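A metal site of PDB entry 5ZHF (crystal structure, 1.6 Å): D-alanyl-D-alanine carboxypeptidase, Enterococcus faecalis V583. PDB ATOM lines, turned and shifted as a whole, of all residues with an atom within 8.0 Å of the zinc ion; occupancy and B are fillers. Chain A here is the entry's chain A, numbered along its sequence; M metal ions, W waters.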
ATOM      1  N   SER A  95      30.363 -19.237  -3.427  1.00  0.00           N
ATOM      2  CA  SER A  95      29.086 -18.846  -3.993  1.00  0.00           C
ATOM      3  C   SER A  95      28.123 -18.476  -2.877  1.00  0.00           C
ATOM      4  O   SER A  95      27.917 -19.263  -1.941  1.00  0.00           O
ATOM      5  CB  SER A  95      28.471 -20.002  -4.796  1.00  0.00           C
ATOM      6  OG  SER A  95      27.201 -19.621  -5.335  1.00  0.00           O
ATOM      7  N   GLY A  96      27.535 -17.295  -2.995  1.00  0.00           N
ATOM      8  CA  GLY A  96      26.506 -16.838  -2.038  1.00  0.00           C
ATOM      9  C   GLY A  96      25.152 -16.755  -2.758  1.00  0.00           C
ATOM     10  O   GLY A  96      24.618 -17.748  -3.264  1.00  0.00           O
ATOM     11  N   ARG A  98      22.392 -16.141  -5.511  1.00  0.00           N
ATOM     12  CA  ARG A  98      22.270 -16.348  -6.939  1.00  0.00           C
ATOM     13  C   ARG A  98      20.919 -15.859  -7.433  1.00  0.00           C
ATOM     14  O   ARG A  98      19.899 -16.104  -6.787  1.00  0.00           O
ATOM     15  CB  ARG A  98      22.353 -17.837  -7.280  1.00  0.00           C
ATOM     16  CG  ARG A  98      23.660 -18.501  -6.941  1.00  0.00           C
ATOM     17  CD  ARG A  98      23.526 -19.984  -7.236  1.00  0.00           C
ATOM     18  NE  ARG A  98      24.654 -20.693  -6.694  1.00  0.00           N
ATOM     19  CZ  ARG A  98      24.708 -21.977  -6.410  1.00  0.00           C
ATOM     20  NH1 ARG A  98      23.677 -22.807  -6.637  1.00  0.00           N
ATOM     21  NH2 ARG A  98      25.834 -22.450  -5.864  1.00  0.00           N
ATOM     22  N   GLN A 103      21.165 -19.525 -11.231  1.00  0.00           N
ATOM     23  CA  GLN A 103      20.782 -20.853 -10.788  1.00  0.00           C
ATOM     24  C   GLN A 103      20.490 -21.782 -11.979  1.00  0.00           C
ATOM     25  O   GLN A 103      20.956 -22.919 -11.985  1.00  0.00           O
ATOM     26  CB  GLN A 103      19.568 -20.818  -9.840  1.00  0.00           C
ATOM     27  CG  GLN A 103      19.255 -22.133  -9.157  1.00  0.00           C
ATOM     28  CD  GLN A 103      20.359 -22.645  -8.228  1.00  0.00           C
ATOM     29  OE1 GLN A 103      21.177 -21.886  -7.731  1.00  0.00           O
ATOM     30  NE2 GLN A 103      20.345 -23.957  -7.980  1.00  0.00           N
ATOM     31  N   TRP A 131      22.065 -32.575  -6.912  1.00  0.00           N
ATOM     32  CA  TRP A 131      23.153 -31.633  -6.636  1.00  0.00           C
ATOM     33  C   TRP A 131      22.784 -30.157  -6.705  1.00  0.00           C
ATOM     34  O   TRP A 131      23.237 -29.371  -5.886  1.00  0.00           O
ATOM     35  CB  TRP A 131      24.311 -31.863  -7.610  1.00  0.00           C
ATOM     36  CG  TRP A 131      24.914 -33.238  -7.528  1.00  0.00           C
ATOM     37  CD1 TRP A 131      24.701 -34.270  -8.393  1.00  0.00           C
ATOM     38  CD2 TRP A 131      25.837 -33.722  -6.546  1.00  0.00           C
ATOM     39  NE1 TRP A 131      25.428 -35.374  -8.007  1.00  0.00           N
ATOM     40  CE2 TRP A 131      26.126 -35.073  -6.872  1.00  0.00           C
ATOM     41  CE3 TRP A 131      26.431 -33.168  -5.403  1.00  0.00           C
ATOM     42  CZ2 TRP A 131      27.004 -35.861  -6.107  1.00  0.00           C
ATOM     43  CZ3 TRP A 131      27.289 -33.942  -4.638  1.00  0.00           C
ATOM     44  CH2 TRP A 131      27.566 -35.288  -5.003  1.00  0.00           C
ATOM     45  N   VAL A 132      22.013 -29.777  -7.718  1.00  0.00           N
ATOM     46  CA  VAL A 132      21.710 -28.377  -8.015  1.00  0.00           C
ATOM     47  C   VAL A 132      20.210 -28.251  -8.138  1.00  0.00           C
ATOM     48  O   VAL A 132      19.582 -28.959  -8.929  1.00  0.00           O
ATOM     49  CB  VAL A 132      22.365 -27.912  -9.335  1.00  0.00           C
ATOM     50  CG1 VAL A 132      22.083 -26.421  -9.592  1.00  0.00           C
ATOM     51  CG2 VAL A 132      23.877 -28.170  -9.335  1.00  0.00           C
ATOM     52  N   SER A 138      16.379 -23.124  -4.729  1.00  0.00           N
ATOM     53  CA  SER A 138      17.725 -23.115  -4.149  1.00  0.00           C
ATOM     54  C   SER A 138      17.783 -22.182  -2.965  1.00  0.00           C
ATOM     55  O   SER A 138      17.335 -21.045  -3.064  1.00  0.00           O
ATOM     56  CB  SER A 138      18.767 -22.607  -5.146  1.00  0.00           C
ATOM     57  OG  SER A 138      20.048 -22.607  -4.505  1.00  0.00           O
ATOM     58  N   GLU A 139      18.407 -22.623  -1.875  1.00  0.00           N
ATOM     59  CA  GLU A 139      18.702 -21.735  -0.791  1.00  0.00           C
ATOM     60  C   GLU A 139      19.610 -20.594  -1.231  1.00  0.00           C
ATOM     61  O   GLU A 139      19.660 -19.572  -0.566  1.00  0.00           O
ATOM     62  CB  GLU A 139      19.408 -22.447   0.358  1.00  0.00           C
ATOM     63  CG  GLU A 139      18.553 -23.434   1.110  1.00  0.00           C
ATOM     64  CD  GLU A 139      19.245 -23.965   2.333  1.00  0.00           C
ATOM     65  OE1 GLU A 139      20.495 -24.112   2.344  1.00  0.00           O
ATOM     66  OE2 GLU A 139      18.538 -24.234   3.322  1.00  0.00           O
ATOM     67  N   HIS A 140      20.383 -20.774  -2.293  1.00  0.00           N
ATOM     68  CA  HIS A 140      21.228 -19.678  -2.754  1.00  0.00           C
ATOM     69  C   HIS A 140      20.425 -18.462  -3.173  1.00  0.00           C
ATOM     70  O   HIS A 140      20.921 -17.350  -3.099  1.00  0.00           O
ATOM     71  CB  HIS A 140      22.182 -20.108  -3.846  1.00  0.00           C
ATOM     72  CG  HIS A 140      23.295 -20.961  -3.344  1.00  0.00           C
ATOM     73  ND1 HIS A 140      24.460 -20.435  -2.831  1.00  0.00           N
ATOM     74  CD2 HIS A 140      23.427 -22.313  -3.255  1.00  0.00           C
ATOM     75  CE1 HIS A 140      25.257 -21.421  -2.453  1.00  0.00           C
ATOM     76  NE2 HIS A 140      24.659 -22.564  -2.699  1.00  0.00           N
ATOM     77  N   ALA A 145      22.513 -18.861   2.177  1.00  0.00           N
ATOM     78  CA  ALA A 145      23.425 -19.990   1.984  1.00  0.00           C
ATOM     79  C   ALA A 145      24.694 -19.569   1.309  1.00  0.00           C
ATOM     80  O   ALA A 145      24.697 -18.701   0.410  1.00  0.00           O
ATOM     81  CB  ALA A 145      22.774 -21.099   1.154  1.00  0.00           C
ATOM     82  N   VAL A 146      25.765 -20.192   1.757  1.00  0.00           N
ATOM     83  CA  VAL A 146      27.074 -19.988   1.164  1.00  0.00           C
ATOM     84  C   VAL A 146      27.727 -21.326   0.878  1.00  0.00           C
ATOM     85  O   VAL A 146      27.673 -22.233   1.699  1.00  0.00           O
ATOM     86  CB  VAL A 146      27.988 -19.096   2.041  1.00  0.00           C
ATOM     87  CG1 VAL A 146      27.555 -17.640   1.973  1.00  0.00           C
ATOM     88  CG2 VAL A 146      28.059 -19.580   3.481  1.00  0.00           C
ATOM     89  N   ASP A 147      28.364 -21.432  -0.293  1.00  0.00           N
ATOM     90  CA  ASP A 147      29.270 -22.554  -0.537  1.00  0.00           C
ATOM     91  C   ASP A 147      30.632 -22.087  -0.118  1.00  0.00           C
ATOM     92  O   ASP A 147      31.113 -21.075  -0.602  1.00  0.00           O
ATOM     93  CB  ASP A 147      29.279 -22.968  -1.996  1.00  0.00           C
ATOM     94  CG  ASP A 147      27.941 -23.477  -2.462  1.00  0.00           C
ATOM     95  OD1 ASP A 147      27.170 -24.060  -1.654  1.00  0.00           O
ATOM     96  OD2 ASP A 147      27.680 -23.348  -3.660  1.00  0.00           O
ATOM     97  N   ILE A 148      31.209 -22.796   0.836  1.00  0.00           N
ATOM     98  CA  ILE A 148      32.457 -22.388   1.434  1.00  0.00           C
ATOM     99  C   ILE A 148      33.481 -23.410   0.982  1.00  0.00           C
ATOM    100  O   ILE A 148      33.301 -24.597   1.207  1.00  0.00           O
ATOM    101  CB  ILE A 148      32.371 -22.340   2.974  1.00  0.00           C
ATOM    102  CG1 ILE A 148      31.320 -21.284   3.403  1.00  0.00           C
ATOM    103  CG2 ILE A 148      33.761 -21.992   3.539  1.00  0.00           C
ATOM    104  CD1 ILE A 148      30.975 -21.362   4.893  1.00  0.00           C
ATOM    105  N   ARG A 176      24.034 -28.176   5.642  1.00  0.00           N
ATOM    106  CA  ARG A 176      22.636 -28.291   5.249  1.00  0.00           C
ATOM    107  C   ARG A 176      22.257 -29.652   4.696  1.00  0.00           C
ATOM    108  O   ARG A 176      21.112 -30.096   4.856  1.00  0.00           O
ATOM    109  CB  ARG A 176      22.338 -27.250   4.196  1.00  0.00           C
ATOM    110  CG  ARG A 176      20.911 -27.199   3.709  1.00  0.00           C
ATOM    111  CD  ARG A 176      19.955 -26.883   4.824  1.00  0.00           C
ATOM    112  NE  ARG A 176      18.588 -26.806   4.351  1.00  0.00           N
ATOM    113  CZ  ARG A 176      17.754 -27.848   4.228  1.00  0.00           C
ATOM    114  NH1 ARG A 176      18.155 -29.097   4.465  1.00  0.00           N
ATOM    115  NH2 ARG A 176      16.500 -27.625   3.834  1.00  0.00           N
ATOM    116  N   TYR A 177      23.198 -30.272   3.991  1.00  0.00           N
ATOM    117  CA  TYR A 177      22.944 -31.517   3.245  1.00  0.00           C
ATOM    118  C   TYR A 177      23.932 -32.603   3.681  1.00  0.00           C
ATOM    119  O   TYR A 177      24.841 -32.960   2.944  1.00  0.00           O
ATOM    120  CB  TYR A 177      23.041 -31.253   1.757  1.00  0.00           C
ATOM    121  CG  TYR A 177      22.131 -30.154   1.235  1.00  0.00           C
ATOM    122  CD1 TYR A 177      20.748 -30.204   1.443  1.00  0.00           C
ATOM    123  CD2 TYR A 177      22.655 -29.035   0.567  1.00  0.00           C
ATOM    124  CE1 TYR A 177      19.917 -29.207   0.957  1.00  0.00           C
ATOM    125  CE2 TYR A 177      21.825 -28.029   0.085  1.00  0.00           C
ATOM    126  CZ  TYR A 177      20.463 -28.106   0.298  1.00  0.00           C
ATOM    127  OH  TYR A 177      19.640 -27.097  -0.196  1.00  0.00           O
ATOM    128  N   VAL A 187      19.072 -34.306  -1.355  1.00  0.00           N
ATOM    129  CA  VAL A 187      20.293 -33.717  -1.894  1.00  0.00           C
ATOM    130  C   VAL A 187      21.491 -34.555  -1.457  1.00  0.00           C
ATOM    131  O   VAL A 187      21.562 -35.016  -0.309  1.00  0.00           O
ATOM    132  CB  VAL A 187      20.434 -32.244  -1.415  1.00  0.00           C
ATOM    133  CG1 VAL A 187      21.699 -31.595  -1.966  1.00  0.00           C
ATOM    134  CG2 VAL A 187      19.191 -31.441  -1.819  1.00  0.00           C
ATOM    135  N   GLU A 190      26.987 -32.487   0.162  1.00  0.00           N
ATOM    136  CA  GLU A 190      27.610 -31.252  -0.300  1.00  0.00           C
ATOM    137  C   GLU A 190      28.293 -30.569   0.889  1.00  0.00           C
ATOM    138  O   GLU A 190      27.742 -29.666   1.520  1.00  0.00           O
ATOM    139  CB  GLU A 190      26.541 -30.340  -0.937  1.00  0.00           C
ATOM    140  CG  GLU A 190      25.930 -30.991  -2.168  1.00  0.00           C
ATOM    141  CD  GLU A 190      25.025 -30.085  -2.946  1.00  0.00           C
ATOM    142  OE1 GLU A 190      24.446 -29.135  -2.377  1.00  0.00           O
ATOM    143  OE2 GLU A 190      24.879 -30.354  -4.145  1.00  0.00           O
ATOM    144  N   TRP A 192      30.456 -28.435   1.308  1.00  0.00           N
ATOM    145  CA  TRP A 192      30.650 -26.998   1.131  1.00  0.00           C
ATOM    146  C   TRP A 192      29.423 -26.120   1.455  1.00  0.00           C
ATOM    147  O   TRP A 192      29.593 -24.919   1.674  1.00  0.00           O
ATOM    148  CB  TRP A 192      31.068 -26.689  -0.324  1.00  0.00           C
ATOM    149  CG  TRP A 192      30.179 -27.300  -1.321  1.00  0.00           C
ATOM    150  CD1 TRP A 192      29.015 -26.788  -1.830  1.00  0.00           C
ATOM    151  CD2 TRP A 192      30.347 -28.585  -1.965  1.00  0.00           C
ATOM    152  NE1 TRP A 192      28.468 -27.661  -2.721  1.00  0.00           N
ATOM    153  CE2 TRP A 192      29.255 -28.777  -2.816  1.00  0.00           C
ATOM    154  CE3 TRP A 192      31.309 -29.592  -1.880  1.00  0.00           C
ATOM    155  CZ2 TRP A 192      29.110 -29.920  -3.610  1.00  0.00           C
ATOM    156  CZ3 TRP A 192      31.150 -30.740  -2.650  1.00  0.00           C
ATOM    157  CH2 TRP A 192      30.078 -30.876  -3.518  1.00  0.00           C
ATOM    158  N   HIS A 193      28.220 -26.688   1.439  1.00  0.00           N
ATOM    159  CA  HIS A 193      26.996 -25.850   1.433  1.00  0.00           C
ATOM    160  C   HIS A 193      26.466 -25.639   2.869  1.00  0.00           C
ATOM    161  O   HIS A 193      25.975 -26.579   3.497  1.00  0.00           O
ATOM    162  CB  HIS A 193      25.919 -26.459   0.538  1.00  0.00           C
ATOM    163  CG  HIS A 193      24.667 -25.644   0.453  1.00  0.00           C
ATOM    164  ND1 HIS A 193      24.292 -24.957  -0.681  1.00  0.00           N
ATOM    165  CD2 HIS A 193      23.705 -25.414   1.380  1.00  0.00           C
ATOM    166  CE1 HIS A 193      23.138 -24.350  -0.453  1.00  0.00           C
ATOM    167  NE2 HIS A 193      22.747 -24.637   0.791  1.00  0.00           N
ATOM    168  N   TYR A 194      26.612 -24.416   3.360  1.00  0.00           N
ATOM    169  CA  TYR A 194      26.229 -24.000   4.710  1.00  0.00           C
ATOM    170  C   TYR A 194      25.084 -22.976   4.675  1.00  0.00           C
ATOM    171  O   TYR A 194      25.078 -22.048   3.858  1.00  0.00           O
ATOM    172  CB  TYR A 194      27.466 -23.509   5.511  1.00  0.00           C
ATOM    173  CG  TYR A 194      28.185 -24.732   6.031  1.00  0.00           C
ATOM    174  CD1 TYR A 194      28.972 -25.512   5.187  1.00  0.00           C
ATOM    175  CD2 TYR A 194      27.978 -25.190   7.331  1.00  0.00           C
ATOM    176  CE1 TYR A 194      29.580 -26.683   5.649  1.00  0.00           C
ATOM    177  CE2 TYR A 194      28.570 -26.351   7.802  1.00  0.00           C
ATOM    178  CZ  TYR A 194      29.355 -27.118   6.952  1.00  0.00           C
ATOM    179  OH  TYR A 194      29.886 -28.280   7.463  1.00  0.00           O
HETATM  180 ZN    ZN M   1      25.349 -24.519  -2.312  1.00  0.00          ZN
HETATM  181  O   HOH W   1      25.572 -26.335  -3.582  1.00  0.00           O
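Water W1 bridges the side-chain carboxylate of Glu 190 (3.2 Å) and the indole nitrogen of Trp 192 (3.3 Å).
Three residues have an atom within 4 Å of the zinc ion: His 140, Asp 147 and His 193.
O of Ser 95 sits at hydrogen-bond distance from N of Asp 147 (2.8 Å).
NE2 of His 193 sits at hydrogen-bond distance from OE1 of Glu 139 (2.8 Å).
The backbone NH (N) of Arg 176 sits at hydrogen-bond distance from the backbone carbonyl oxygen (O) of His 193, at 3.3 Å.
The backbone NH (N) of His 140 is in hydrogen-bond range of the side-chain hydroxyl (OG) of Ser 138 (2.9 Å).
The side-chain carboxylate of Asp 147 lies within salt-bridge range of the guanidinium group of Arg 98, at 3.0 Å.
The backbone NH of Arg 98 sits at hydrogen-bond distance from the backbone carbonyl oxygen of His 140.
ND1 of His 140 sits at hydrogen-bond distance from O of Gly 96 (2.7 Å).
OD1 of Asp 147 binds the zinc ion.
ND1 of His 193 is bound to the zinc ion (2.0 Å).
NE2 of His 140 is bound to the zinc ion (2.1 Å).
Water W1 binds the zinc ion (2.2 Å).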
